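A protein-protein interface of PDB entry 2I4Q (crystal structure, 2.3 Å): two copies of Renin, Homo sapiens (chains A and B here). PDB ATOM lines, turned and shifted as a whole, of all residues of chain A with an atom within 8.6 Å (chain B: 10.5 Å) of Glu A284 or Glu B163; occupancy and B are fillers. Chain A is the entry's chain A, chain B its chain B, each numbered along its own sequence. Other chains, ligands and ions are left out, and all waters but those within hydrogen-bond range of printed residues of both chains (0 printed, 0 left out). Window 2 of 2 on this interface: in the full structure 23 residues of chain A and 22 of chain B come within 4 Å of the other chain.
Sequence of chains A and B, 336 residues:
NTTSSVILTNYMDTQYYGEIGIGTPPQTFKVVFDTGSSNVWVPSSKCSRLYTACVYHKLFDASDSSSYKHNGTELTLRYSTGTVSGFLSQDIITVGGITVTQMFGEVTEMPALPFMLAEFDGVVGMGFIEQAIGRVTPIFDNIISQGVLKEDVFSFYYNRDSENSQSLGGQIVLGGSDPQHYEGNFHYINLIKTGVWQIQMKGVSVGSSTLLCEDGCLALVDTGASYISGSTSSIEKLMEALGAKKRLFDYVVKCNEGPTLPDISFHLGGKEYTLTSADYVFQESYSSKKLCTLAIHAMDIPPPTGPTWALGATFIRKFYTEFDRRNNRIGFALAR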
ATOM      1  N   MET A  12       8.171   2.728  -8.816  1.00  0.00           N
ATOM      2  CA  MET A  12       7.786   1.384  -8.352  1.00  0.00           C
ATOM      3  C   MET A  12       6.722   0.688  -9.203  1.00  0.00           C
ATOM      4  O   MET A  12       6.010  -0.188  -8.714  1.00  0.00           O
ATOM      5  CB  MET A  12       7.319   1.448  -6.889  1.00  0.00           C
ATOM      6  CG  MET A  12       8.370   2.020  -5.941  1.00  0.00           C
ATOM      7  SD  MET A  12       8.187   1.492  -4.216  1.00  0.00           S
ATOM      8  CE  MET A  12       6.370   1.486  -4.021  1.00  0.00           C
ATOM      9  N   GLU A 163      16.403  -0.107 -11.850  1.00  0.00           N
ATOM     10  CA  GLU A 163      17.282   0.230 -10.729  1.00  0.00           C
ATOM     11  C   GLU A 163      18.154   1.456 -11.030  1.00  0.00           C
ATOM     12  O   GLU A 163      18.507   2.204 -10.115  1.00  0.00           O
ATOM     13  CB  GLU A 163      18.168  -0.965 -10.356  1.00  0.00           C
ATOM     14  CG  GLU A 163      17.396  -2.160  -9.804  1.00  0.00           C
ATOM     15  CD  GLU A 163      18.193  -2.971  -8.795  1.00  0.00           C
ATOM     16  OE1 GLU A 163      17.618  -3.359  -7.752  1.00  0.00           O
ATOM     17  OE2 GLU A 163      19.395  -3.221  -9.048  1.00  0.00           O
ATOM     18  N   ARG A 247      -5.979 -10.377   0.315  1.00  0.00           N
ATOM     19  CA  ARG A 247      -5.489  -9.531   1.397  1.00  0.00           C
ATOM     20  C   ARG A 247      -6.409  -8.310   1.507  1.00  0.00           C
ATOM     21  O   ARG A 247      -7.465  -8.256   0.863  1.00  0.00           O
ATOM     22  CB  ARG A 247      -4.031  -9.114   1.138  1.00  0.00           C
ATOM     23  CG  ARG A 247      -3.088  -9.320   2.320  1.00  0.00           C
ATOM     24  CD  ARG A 247      -1.611  -9.398   1.937  1.00  0.00           C
ATOM     25  NE  ARG A 247      -0.796  -8.375   2.599  1.00  0.00           N
ATOM     26  CZ  ARG A 247       0.539  -8.308   2.541  1.00  0.00           C
ATOM     27  NH1 ARG A 247       1.181  -7.333   3.182  1.00  0.00           N
ATOM     28  NH2 ARG A 247       1.238  -9.205   1.850  1.00  0.00           N
ATOM     29  N   VAL A 252      -2.531 -11.642  -3.428  1.00  0.00           N
ATOM     30  CA  VAL A 252      -1.161 -12.152  -3.360  1.00  0.00           C
ATOM     31  C   VAL A 252      -1.083 -13.648  -3.638  1.00  0.00           C
ATOM     32  O   VAL A 252      -2.026 -14.383  -3.379  1.00  0.00           O
ATOM     33  CB  VAL A 252      -0.521 -11.902  -1.972  1.00  0.00           C
ATOM     34  CG1 VAL A 252      -0.415 -10.418  -1.685  1.00  0.00           C
ATOM     35  CG2 VAL A 252      -1.297 -12.628  -0.854  1.00  0.00           C
ATOM     36  N   CYS A 255       5.416 -16.309  -3.315  1.00  0.00           N
ATOM     37  CA  CYS A 255       6.348 -15.731  -4.286  1.00  0.00           C
ATOM     38  C   CYS A 255       6.911 -16.768  -5.262  1.00  0.00           C
ATOM     39  O   CYS A 255       7.126 -16.460  -6.433  1.00  0.00           O
ATOM     40  CB  CYS A 255       7.491 -14.988  -3.583  1.00  0.00           C
ATOM     41  SG  CYS A 255       7.099 -13.288  -3.116  1.00  0.00           S
ATOM     42  N   ASN A 256       7.133 -17.988  -4.778  1.00  0.00           N
ATOM     43  CA  ASN A 256       7.619 -19.084  -5.620  1.00  0.00           C
ATOM     44  C   ASN A 256       6.619 -19.528  -6.700  1.00  0.00           C
ATOM     45  O   ASN A 256       7.010 -20.057  -7.739  1.00  0.00           O
ATOM     46  CB  ASN A 256       8.017 -20.285  -4.752  1.00  0.00           C
ATOM     47  CG  ASN A 256       6.819 -20.998  -4.151  1.00  0.00           C
ATOM     48  OD1 ASN A 256       6.159 -20.474  -3.256  1.00  0.00           O
ATOM     49  ND2 ASN A 256       6.528 -22.194  -4.649  1.00  0.00           N
ATOM     50  N   GLY A 258       4.681 -17.457  -8.360  1.00  0.00           N
ATOM     51  CA  GLY A 258       4.516 -16.359  -9.300  1.00  0.00           C
ATOM     52  C   GLY A 258       4.805 -16.650 -10.763  1.00  0.00           C
ATOM     53  O   GLY A 258       3.944 -16.420 -11.606  1.00  0.00           O
ATOM     54  N   PRO A 259       6.006 -17.133 -11.080  1.00  0.00           N
ATOM     55  CA  PRO A 259       6.381 -17.425 -12.470  1.00  0.00           C
ATOM     56  C   PRO A 259       5.538 -18.503 -13.176  1.00  0.00           C
ATOM     57  O   PRO A 259       5.528 -18.519 -14.403  1.00  0.00           O
ATOM     58  CB  PRO A 259       7.837 -17.884 -12.343  1.00  0.00           C
ATOM     59  CG  PRO A 259       8.300 -17.310 -11.059  1.00  0.00           C
ATOM     60  CD  PRO A 259       7.120 -17.405 -10.153  1.00  0.00           C
ATOM     61  N   VAL A 281       2.661  -9.947 -11.963  1.00  0.00           N
ATOM     62  CA  VAL A 281       3.091 -10.154 -10.580  1.00  0.00           C
ATOM     63  C   VAL A 281       4.345  -9.329 -10.328  1.00  0.00           C
ATOM     64  O   VAL A 281       5.226  -9.239 -11.178  1.00  0.00           O
ATOM     65  CB  VAL A 281       3.275 -11.671 -10.158  1.00  0.00           C
ATOM     66  CG1 VAL A 281       2.703 -12.633 -11.181  1.00  0.00           C
ATOM     67  CG2 VAL A 281       4.724 -12.017  -9.844  1.00  0.00           C
ATOM     68  N   PHE A 282       4.380  -8.706  -9.156  1.00  0.00           N
ATOM     69  CA  PHE A 282       5.559  -8.028  -8.654  1.00  0.00           C
ATOM     70  C   PHE A 282       6.478  -9.081  -8.078  1.00  0.00           C
ATOM     71  O   PHE A 282       6.427  -9.369  -6.884  1.00  0.00           O
ATOM     72  CB  PHE A 282       5.175  -7.019  -7.568  1.00  0.00           C
ATOM     73  CG  PHE A 282       4.483  -5.811  -8.091  1.00  0.00           C
ATOM     74  CD1 PHE A 282       3.130  -5.854  -8.404  1.00  0.00           C
ATOM     75  CD2 PHE A 282       5.179  -4.624  -8.277  1.00  0.00           C
ATOM     76  CE1 PHE A 282       2.480  -4.730  -8.896  1.00  0.00           C
ATOM     77  CE2 PHE A 282       4.537  -3.500  -8.770  1.00  0.00           C
ATOM     78  CZ  PHE A 282       3.185  -3.552  -9.080  1.00  0.00           C
ATOM     79  N   GLN A 283       7.296  -9.673  -8.940  1.00  0.00           N
ATOM     80  CA  GLN A 283       8.225 -10.721  -8.539  1.00  0.00           C
ATOM     81  C   GLN A 283       9.394 -10.125  -7.745  1.00  0.00           C
ATOM     82  O   GLN A 283      10.455  -9.833  -8.297  1.00  0.00           O
ATOM     83  CB  GLN A 283       8.712 -11.492  -9.777  1.00  0.00           C
ATOM     84  CG  GLN A 283       9.108 -12.937  -9.515  1.00  0.00           C
ATOM     85  CD  GLN A 283       7.956 -13.783  -9.002  1.00  0.00           C
ATOM     86  OE1 GLN A 283       7.049 -14.138  -9.757  1.00  0.00           O
ATOM     87  NE2 GLN A 283       7.985 -14.099  -7.715  1.00  0.00           N
ATOM     88  N   GLU A 284       9.173  -9.948  -6.441  1.00  0.00           N
ATOM     89  CA  GLU A 284      10.163  -9.382  -5.525  1.00  0.00           C
ATOM     90  C   GLU A 284      11.059 -10.476  -4.951  1.00  0.00           C
ATOM     91  O   GLU A 284      12.050 -10.185  -4.284  1.00  0.00           O
ATOM     92  CB  GLU A 284       9.471  -8.684  -4.345  1.00  0.00           C
ATOM     93  CG  GLU A 284       8.701  -7.415  -4.691  1.00  0.00           C
ATOM     94  CD  GLU A 284       7.813  -6.929  -3.546  1.00  0.00           C
ATOM     95  OE1 GLU A 284       7.324  -5.776  -3.617  1.00  0.00           O
ATOM     96  OE2 GLU A 284       7.588  -7.695  -2.575  1.00  0.00           O
ATOM     97  N   SER A 285      10.685 -11.731  -5.184  1.00  0.00           N
ATOM     98  CA  SER A 285      11.358 -12.870  -4.574  1.00  0.00           C
ATOM     99  C   SER A 285      10.883 -14.177  -5.199  1.00  0.00           C
ATOM    100  O   SER A 285       9.895 -14.206  -5.929  1.00  0.00           O
ATOM    101  CB  SER A 285      11.078 -12.904  -3.068  1.00  0.00           C
ATOM    102  OG  SER A 285      12.116 -13.570  -2.372  1.00  0.00           O
ATOM    103  N   TYR A 286      11.594 -15.257  -4.903  1.00  0.00           N
ATOM    104  CA  TYR A 286      11.183 -16.592  -5.317  1.00  0.00           C
ATOM    105  C   TYR A 286      10.927 -17.468  -4.093  1.00  0.00           C
ATOM    106  O   TYR A 286      10.810 -18.688  -4.205  1.00  0.00           O
ATOM    107  CB  TYR A 286      12.264 -17.214  -6.204  1.00  0.00           C
ATOM    108  CG  TYR A 286      12.583 -16.399  -7.442  1.00  0.00           C
ATOM    109  CD1 TYR A 286      11.677 -16.318  -8.498  1.00  0.00           C
ATOM    110  CD2 TYR A 286      13.792 -15.709  -7.559  1.00  0.00           C
ATOM    111  CE1 TYR A 286      11.963 -15.573  -9.641  1.00  0.00           C
ATOM    112  CE2 TYR A 286      14.088 -14.963  -8.700  1.00  0.00           C
ATOM    113  CZ  TYR A 286      13.170 -14.901  -9.734  1.00  0.00           C
ATOM    114  OH  TYR A 286      13.452 -14.169 -10.863  1.00  0.00           O
ATOM    115  N   SER A 287      10.817 -16.831  -2.931  1.00  0.00           N
ATOM    116  CA  SER A 287      10.711 -17.535  -1.657  1.00  0.00           C
ATOM    117  C   SER A 287       9.276 -17.991  -1.412  1.00  0.00           C
ATOM    118  O   SER A 287       8.342 -17.220  -1.597  1.00  0.00           O
ATOM    119  CB  SER A 287      11.172 -16.613  -0.516  1.00  0.00           C
ATOM    120  OG  SER A 287      10.961 -17.198   0.760  1.00  0.00           O
ATOM    121  N   LYS A 290       7.866 -15.667   1.546  1.00  0.00           N
ATOM    122  CA  LYS A 290       7.429 -14.297   1.261  1.00  0.00           C
ATOM    123  C   LYS A 290       6.176 -14.289   0.384  1.00  0.00           C
ATOM    124  O   LYS A 290       5.909 -15.249  -0.337  1.00  0.00           O
ATOM    125  CB  LYS A 290       8.543 -13.501   0.573  1.00  0.00           C
ATOM    126  CG  LYS A 290       9.712 -13.135   1.488  1.00  0.00           C
ATOM    127  CD  LYS A 290      10.981 -12.840   0.678  1.00  0.00           C
ATOM    128  CE  LYS A 290      12.028 -12.066   1.482  1.00  0.00           C
ATOM    129  NZ  LYS A 290      12.305 -10.720   0.896  1.00  0.00           N
ATOM    130  N   LEU A 291       5.417 -13.198   0.458  1.00  0.00           N
ATOM    131  CA  LEU A 291       4.213 -13.007  -0.352  1.00  0.00           C
ATOM    132  C   LEU A 291       4.467 -11.973  -1.450  1.00  0.00           C
ATOM    133  O   LEU A 291       5.154 -10.981  -1.224  1.00  0.00           O
ATOM    134  CB  LEU A 291       3.046 -12.546   0.532  1.00  0.00           C
ATOM    135  CG  LEU A 291       2.541 -13.540   1.584  1.00  0.00           C
ATOM    136  CD1 LEU A 291       1.576 -12.861   2.541  1.00  0.00           C
ATOM    137  CD2 LEU A 291       1.884 -14.748   0.931  1.00  0.00           C
ATOM    138  N   CYS A 292       3.906 -12.216  -2.634  1.00  0.00           N
ATOM    139  CA  CYS A 292       4.088 -11.344  -3.793  1.00  0.00           C
ATOM    140  C   CYS A 292       2.750 -10.803  -4.280  1.00  0.00           C
ATOM    141  O   CYS A 292       1.798 -11.559  -4.467  1.00  0.00           O
ATOM    142  CB  CYS A 292       4.786 -12.104  -4.925  1.00  0.00           C
ATOM    143  SG  CYS A 292       6.586 -12.184  -4.750  1.00  0.00           S
ATOM    144  N   THR A 293       2.690  -9.491  -4.493  1.00  0.00           N
ATOM    145  CA  THR A 293       1.468  -8.821  -4.922  1.00  0.00           C
ATOM    146  C   THR A 293       1.246  -8.953  -6.427  1.00  0.00           C
ATOM    147  O   THR A 293       2.198  -8.998  -7.205  1.00  0.00           O
ATOM    148  CB  THR A 293       1.530  -7.333  -4.550  1.00  0.00           C
ATOM    149  OG1 THR A 293       1.819  -7.193  -3.153  1.00  0.00           O
ATOM    150  CG2 THR A 293       0.170  -6.666  -4.713  1.00  0.00           C
ATOM    151  N   ASN B  10      14.082 -12.801 -16.722  1.00  0.00           N
ATOM    152  CA  ASN B  10      15.191 -13.450 -16.037  1.00  0.00           C
ATOM    153  C   ASN B  10      14.697 -14.202 -14.809  1.00  0.00           C
ATOM    154  O   ASN B  10      14.308 -13.591 -13.825  1.00  0.00           O
ATOM    155  CB  ASN B  10      16.242 -12.421 -15.618  1.00  0.00           C
ATOM    156  CG  ASN B  10      17.365 -13.034 -14.785  1.00  0.00           C
ATOM    157  OD1 ASN B  10      17.300 -14.200 -14.405  1.00  0.00           O
ATOM    158  ND2 ASN B  10      18.401 -12.248 -14.508  1.00  0.00           N
ATOM    159  N   TYR B  11      14.742 -15.526 -14.870  1.00  0.00           N
ATOM    160  CA  TYR B  11      14.481 -16.373 -13.714  1.00  0.00           C
ATOM    161  C   TYR B  11      15.785 -16.847 -13.067  1.00  0.00           C
ATOM    162  O   TYR B  11      16.482 -17.690 -13.619  1.00  0.00           O
ATOM    163  CB  TYR B  11      13.651 -17.584 -14.144  1.00  0.00           C
ATOM    164  CG  TYR B  11      13.360 -18.557 -13.025  1.00  0.00           C
ATOM    165  CD1 TYR B  11      12.417 -18.259 -12.054  1.00  0.00           C
ATOM    166  CD2 TYR B  11      14.026 -19.770 -12.943  1.00  0.00           C
ATOM    167  CE1 TYR B  11      12.143 -19.145 -11.016  1.00  0.00           C
ATOM    168  CE2 TYR B  11      13.760 -20.676 -11.907  1.00  0.00           C
ATOM    169  CZ  TYR B  11      12.817 -20.354 -10.953  1.00  0.00           C
ATOM    170  OH  TYR B  11      12.550 -21.225  -9.934  1.00  0.00           O
ATOM    171  N   MET B  12      16.105 -16.297 -11.898  1.00  0.00           N
ATOM    172  CA  MET B  12      17.215 -16.762 -11.049  1.00  0.00           C
ATOM    173  C   MET B  12      18.611 -16.745 -11.705  1.00  0.00           C
ATOM    174  O   MET B  12      19.524 -17.446 -11.260  1.00  0.00           O
ATOM    175  CB  MET B  12      16.906 -18.164 -10.503  1.00  0.00           C
ATOM    176  CG  MET B  12      15.918 -18.186  -9.342  1.00  0.00           C
ATOM    177  SD  MET B  12      15.490 -19.872  -8.819  1.00  0.00           S
ATOM    178  CE  MET B  12      17.054 -20.494  -8.393  1.00  0.00           C
ATOM    179  N   ASP B  13      18.779 -15.929 -12.747  1.00  0.00           N
ATOM    180  CA  ASP B  13      20.039 -15.840 -13.488  1.00  0.00           C
ATOM    181  C   ASP B  13      20.434 -17.124 -14.250  1.00  0.00           C
ATOM    182  O   ASP B  13      21.575 -17.249 -14.675  1.00  0.00           O
ATOM    183  CB  ASP B  13      21.187 -15.431 -12.536  1.00  0.00           C
ATOM    184  CG  ASP B  13      21.438 -13.932 -12.509  1.00  0.00           C
ATOM    185  OD1 ASP B  13      20.569 -13.139 -12.939  1.00  0.00           O
ATOM    186  OD2 ASP B  13      22.504 -13.458 -12.060  1.00  0.00           O
ATOM    187  N   ASN B 159      20.154  -9.315 -18.341  1.00  0.00           N
ATOM    188  CA  ASN B 159      20.327  -8.499 -17.143  1.00  0.00           C
ATOM    189  C   ASN B 159      20.703  -9.336 -15.915  1.00  0.00           C
ATOM    190  O   ASN B 159      20.524 -10.548 -15.906  1.00  0.00           O
ATOM    191  CB  ASN B 159      19.028  -7.720 -16.871  1.00  0.00           C
ATOM    192  CG  ASN B 159      19.217  -6.532 -15.926  1.00  0.00           C
ATOM    193  OD1 ASN B 159      20.330  -6.191 -15.534  1.00  0.00           O
ATOM    194  ND2 ASN B 159      18.116  -5.893 -15.572  1.00  0.00           N
ATOM    195  N   ARG B 160      21.258  -8.677 -14.903  1.00  0.00           N
ATOM    196  CA  ARG B 160      21.450  -9.264 -13.579  1.00  0.00           C
ATOM    197  C   ARG B 160      20.104  -9.316 -12.849  1.00  0.00           C
ATOM    198  O   ARG B 160      19.236  -8.466 -13.059  1.00  0.00           O
ATOM    199  CB  ARG B 160      22.442  -8.430 -12.748  1.00  0.00           C
ATOM    200  CG  ARG B 160      23.906  -8.868 -12.826  1.00  0.00           C
ATOM    201  CD  ARG B 160      24.678  -8.292 -14.000  1.00  0.00           C
ATOM    202  NE  ARG B 160      25.259  -6.978 -13.719  1.00  0.00           N
ATOM    203  CZ  ARG B 160      26.133  -6.343 -14.510  1.00  0.00           C
ATOM    204  NH1 ARG B 160      26.598  -5.148 -14.157  1.00  0.00           N
ATOM    205  NH2 ARG B 160      26.551  -6.889 -15.647  1.00  0.00           N
ATOM    206  N   ASP B 161      19.953 -10.306 -11.974  1.00  0.00           N
ATOM    207  CA  ASP B 161      18.736 -10.466 -11.180  1.00  0.00           C
ATOM    208  C   ASP B 161      18.753  -9.480 -10.016  1.00  0.00           C
ATOM    209  O   ASP B 161      19.791  -9.281  -9.383  1.00  0.00           O
ATOM    210  CB  ASP B 161      18.641 -11.902 -10.651  1.00  0.00           C
ATOM    211  CG  ASP B 161      17.264 -12.248 -10.116  1.00  0.00           C
ATOM    212  OD1 ASP B 161      17.190 -13.140  -9.241  1.00  0.00           O
ATOM    213  OD2 ASP B 161      16.206 -11.707 -10.511  1.00  0.00           O
ATOM    214  N   SER B 162      17.606  -8.856  -9.753  1.00  0.00           N
ATOM    215  CA  SER B 162      17.440  -7.987  -8.587  1.00  0.00           C
ATOM    216  C   SER B 162      16.083  -8.234  -7.924  1.00  0.00           C
ATOM    217  O   SER B 162      15.039  -8.189  -8.581  1.00  0.00           O
ATOM    218  CB  SER B 162      17.584  -6.514  -8.982  1.00  0.00           C
ATOM    219  OG  SER B 162      16.550  -6.107  -9.863  1.00  0.00           O
ATOM    220  N   GLU B 163      16.111  -8.484  -6.617  1.00  0.00           N
ATOM    221  CA  GLU B 163      14.899  -8.796  -5.849  1.00  0.00           C
ATOM    222  C   GLU B 163      14.094  -7.542  -5.442  1.00  0.00           C
ATOM    223  O   GLU B 163      13.009  -7.660  -4.869  1.00  0.00           O
ATOM    224  CB  GLU B 163      15.256  -9.637  -4.606  1.00  0.00           C
ATOM    225  CG  GLU B 163      14.873 -11.114  -4.700  1.00  0.00           C
ATOM    226  CD  GLU B 163      15.855 -11.951  -5.503  1.00  0.00           C
ATOM    227  OE1 GLU B 163      16.625 -12.723  -4.888  1.00  0.00           O
ATOM    228  OE2 GLU B 163      15.845 -11.855  -6.750  1.00  0.00           O
ATOM    229  N   ASN B 164      14.611  -6.351  -5.743  1.00  0.00           N
ATOM    230  CA  ASN B 164      13.936  -5.102  -5.386  1.00  0.00           C
ATOM    231  C   ASN B 164      13.504  -4.280  -6.603  1.00  0.00           C
ATOM    232  O   ASN B 164      13.446  -3.050  -6.543  1.00  0.00           O
ATOM    233  CB  ASN B 164      14.839  -4.274  -4.466  1.00  0.00           C
ATOM    234  CG  ASN B 164      14.929  -4.857  -3.068  1.00  0.00           C
ATOM    235  OD1 ASN B 164      14.007  -4.705  -2.260  1.00  0.00           O
ATOM    236  ND2 ASN B 164      16.034  -5.544  -2.780  1.00  0.00           N
ATOM    237  N   SER B 165      13.193  -4.966  -7.703  1.00  0.00           N
ATOM    238  CA  SER B 165      12.685  -4.302  -8.908  1.00  0.00           C
ATOM    239  C   SER B 165      11.880  -5.248  -9.811  1.00  0.00           C
ATOM    240  O   SER B 165      11.944  -6.473  -9.668  1.00  0.00           O
ATOM    241  CB  SER B 165      13.843  -3.674  -9.700  1.00  0.00           C
ATOM    242  OG  SER B 165      13.562  -2.326 -10.038  1.00  0.00           O
ATOM    243  N   GLN B 166      11.113  -4.654 -10.725  1.00  0.00           N
ATOM    244  CA  GLN B 166      10.410  -5.386 -11.782  1.00  0.00           C
ATOM    245  C   GLN B 166      11.131  -5.113 -13.095  1.00  0.00           C
ATOM    246  O   GLN B 166      10.523  -4.777 -14.118  1.00  0.00           O
ATOM    247  CB  GLN B 166       8.941  -4.952 -11.856  1.00  0.00           C
ATOM    248  CG  GLN B 166       8.203  -5.036 -10.524  1.00  0.00           C
ATOM    249  CD  GLN B 166       8.530  -6.306  -9.766  1.00  0.00           C
ATOM    250  OE1 GLN B 166       8.893  -6.264  -8.585  1.00  0.00           O
ATOM    251  NE2 GLN B 166       8.421  -7.441 -10.449  1.00  0.00           N
ATOM    252  N   SER B 167      12.446  -5.288 -13.046  1.00  0.00           N
ATOM    253  CA  SER B 167      13.333  -4.820 -14.095  1.00  0.00           C
ATOM    254  C   SER B 167      13.271  -5.688 -15.338  1.00  0.00           C
ATOM    255  O   SER B 167      12.755  -6.803 -15.322  1.00  0.00           O
ATOM    256  CB  SER B 167      14.769  -4.764 -13.578  1.00  0.00           C
ATOM    257  OG  SER B 167      15.598  -4.091 -14.499  1.00  0.00           O
ATOM    258  N   LEU B 168      13.790  -5.134 -16.425  1.00  0.00           N
ATOM    259  CA  LEU B 168      13.969  -5.867 -17.657  1.00  0.00           C
ATOM    260  C   LEU B 168      14.853  -7.076 -17.362  1.00  0.00           C
ATOM    261  O   LEU B 168      15.980  -6.931 -16.883  1.00  0.00           O
ATOM    262  CB  LEU B 168      14.633  -4.960 -18.696  1.00  0.00           C
ATOM    263  CG  LEU B 168      14.473  -5.348 -20.162  1.00  0.00           C
ATOM    264  CD1 LEU B 168      13.042  -5.125 -20.611  1.00  0.00           C
ATOM    265  CD2 LEU B 168      15.436  -4.543 -21.023  1.00  0.00           C
ATOM    266  N   PHE B 282      27.675 -16.521  -7.423  1.00  0.00           N
ATOM    267  CA  PHE B 282      26.316 -16.266  -6.964  1.00  0.00           C
ATOM    268  C   PHE B 282      26.412 -15.933  -5.485  1.00  0.00           C
ATOM    269  O   PHE B 282      26.494 -16.827  -4.638  1.00  0.00           O
ATOM    270  CB  PHE B 282      25.413 -17.480  -7.192  1.00  0.00           C
ATOM    271  CG  PHE B 282      25.144 -17.780  -8.644  1.00  0.00           C
ATOM    272  CD1 PHE B 282      25.458 -19.030  -9.182  1.00  0.00           C
ATOM    273  CD2 PHE B 282      24.565 -16.826  -9.473  1.00  0.00           C
ATOM    274  CE1 PHE B 282      25.199 -19.322 -10.520  1.00  0.00           C
ATOM    275  CE2 PHE B 282      24.306 -17.109 -10.816  1.00  0.00           C
ATOM    276  CZ  PHE B 282      24.626 -18.358 -11.339  1.00  0.00           C
ATOM    277  N   GLN B 283      26.453 -14.639  -5.186  1.00  0.00           N
ATOM    278  CA  GLN B 283      26.570 -14.167  -3.814  1.00  0.00           C
ATOM    279  C   GLN B 283      25.173 -14.017  -3.222  1.00  0.00           C
ATOM    280  O   GLN B 283      24.675 -12.908  -3.069  1.00  0.00           O
ATOM    281  CB  GLN B 283      27.326 -12.833  -3.756  1.00  0.00           C
ATOM    282  CG  GLN B 283      28.772 -12.881  -4.274  1.00  0.00           C
ATOM    283  CD  GLN B 283      29.797 -13.380  -3.246  1.00  0.00           C
ATOM    284  OE1 GLN B 283      30.997 -13.340  -3.508  1.00  0.00           O
ATOM    285  NE2 GLN B 283      29.328 -13.850  -2.091  1.00  0.00           N
ATOM    286  N   GLU B 284      24.547 -15.148  -2.898  1.00  0.00           N
ATOM    287  CA  GLU B 284      23.243 -15.158  -2.231  1.00  0.00           C
ATOM    288  C   GLU B 284      23.345 -14.506  -0.851  1.00  0.00           C
ATOM    289  O   GLU B 284      22.354 -14.004  -0.330  1.00  0.00           O
ATOM    290  CB  GLU B 284      22.703 -16.587  -2.102  1.00  0.00           C
ATOM    291  CG  GLU B 284      22.351 -17.239  -3.435  1.00  0.00           C
ATOM    292  CD  GLU B 284      20.859 -17.446  -3.613  1.00  0.00           C
ATOM    293  OE1 GLU B 284      20.372 -18.581  -3.373  1.00  0.00           O
ATOM    294  OE2 GLU B 284      20.172 -16.471  -3.994  1.00  0.00           O
ATOM    295  N   SER B 285      24.542 -14.554  -0.266  1.00  0.00           N
ATOM    296  CA  SER B 285      24.900 -13.737   0.890  1.00  0.00           C
ATOM    297  C   SER B 285      26.385 -13.393   0.845  1.00  0.00           C
ATOM    298  O   SER B 285      27.071 -13.720  -0.121  1.00  0.00           O
ATOM    299  CB  SER B 285      24.576 -14.479   2.190  1.00  0.00           C
ATOM    300  OG  SER B 285      25.611 -15.390   2.534  1.00  0.00           O
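Printed residues of chain B within 4 Å of Glu A163: Ser B162 (3.4 Å) and Ser B165 (3.8 Å). Cys A255 touches none of the printed residues of chain B. Gln A283 touches just these residues of chain B: Ser B165 and Gln B166. Glu A284 touches just one residue of chain B: Glu B163 (2.8 Å). Of chain B, only Glu B163 (3.9 Å) comes within 4 Å of Ser A285. Of the printed residues of chain B, Tyr A286 touches Asn B10 (3.1 Å), Tyr B11 (3.6 Å), Met B12 (3.6 Å) and Asp B161 (3.6 Å). Arg B160 touches none of the printed residues of chain A. Of the printed residues of chain A, Asp B161 touches Tyr A286 (3.6 Å). Glu B163 touches just these residues of chain A: Glu A284 and Ser A285. Printed residues of chain A within 4 Å of Gln B166: Val A281 (3.7 Å), Phe A282 (3.4 Å) and Gln A283 (2.9 Å). The nearest residue of chain B that does not touch Glu A284 is Gln B166 (4.1 Å). The nearest residue of chain A that does not touch Glu B163 is Tyr A286 (4.1 Å).
Of the 18 printed residues of chain B, 8 touch a printed residue of chain A. Hydrophobic or aromatic side chains of chain B that line the printed part of chain A: Tyr B11 and Met B12. Of the 19 printed residues of chain A, 7 touch a printed residue of chain B. Printed residues of chain A that touch a printed residue of chain B: Glu A163, Val A281, Phe A282, Gln A283, Glu A284, Ser A285 and Tyr A286. Hydrophobic or aromatic side chains of chain A that line the printed part of chain B: Phe A282 and Tyr A286. Among the printed residues, 12 pairs touch across the chains.
Among the printed residues, pairs that only touch across the chains: Glu A163 with Ser B162 (3.4 Å), Phe A282 with Gln B166 (3.4 Å), Tyr A286 with Met B12 (3.6 Å), Tyr A286 with Asp B161 (3.6 Å), Tyr A286 with Tyr B11 (3.6 Å), Val A281 with Gln B166 (3.7 Å), Glu A163 with Ser B165 (3.8 Å), Gln A283 with Ser B165 (3.9 Å) and Ser A285 with Glu B163 (3.9 Å).
The side-chain amide nitrogen (NE2) of Gln A283 sits at hydrogen-bond distance from the backbone carbonyl oxygen (O) of Ser A285, at 2.6 Å. N of Phe A282 is in hydrogen-bond range of O of Thr A293, 2.9 Å away. The backbone NH (N) of Asp B161 is in hydrogen-bond range of the side-chain carboxylate (OD1) of Asp B13 (3.1 Å). The side-chain sulfur of Cys A292 is disulfide-bonded to the side-chain sulfur of Cys A255, 2.0 Å away. The side-chain amide oxygen (OD1) of Asn B10 sits at hydrogen-bond distance from the backbone NH (N) of Asp B13, 2.8 Å away.
Glu A284 touches Glu B163, but with the chains exchanged Glu A163 does not touch Glu B284 (13.8 Å). Ser A285 touches Glu B163, but with the chains exchanged Glu A163 does not touch Ser B285 (15.1 Å). 6 positions are printed for both chains. Of the 12 pairs that touch across the chains among the printed residues, none has its exchanged pair printed and touching as well.
O of Glu B163 sits close to O of Glu A284, 2.8 Å away. OH of Tyr A286 lies within hydrogen-bond range of O of Asn B10, at 3.1 Å. The backbone NH (N) of Gln A283 lies close to the side-chain amide nitrogen (NE2) of Gln B166 (2.9 Å).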
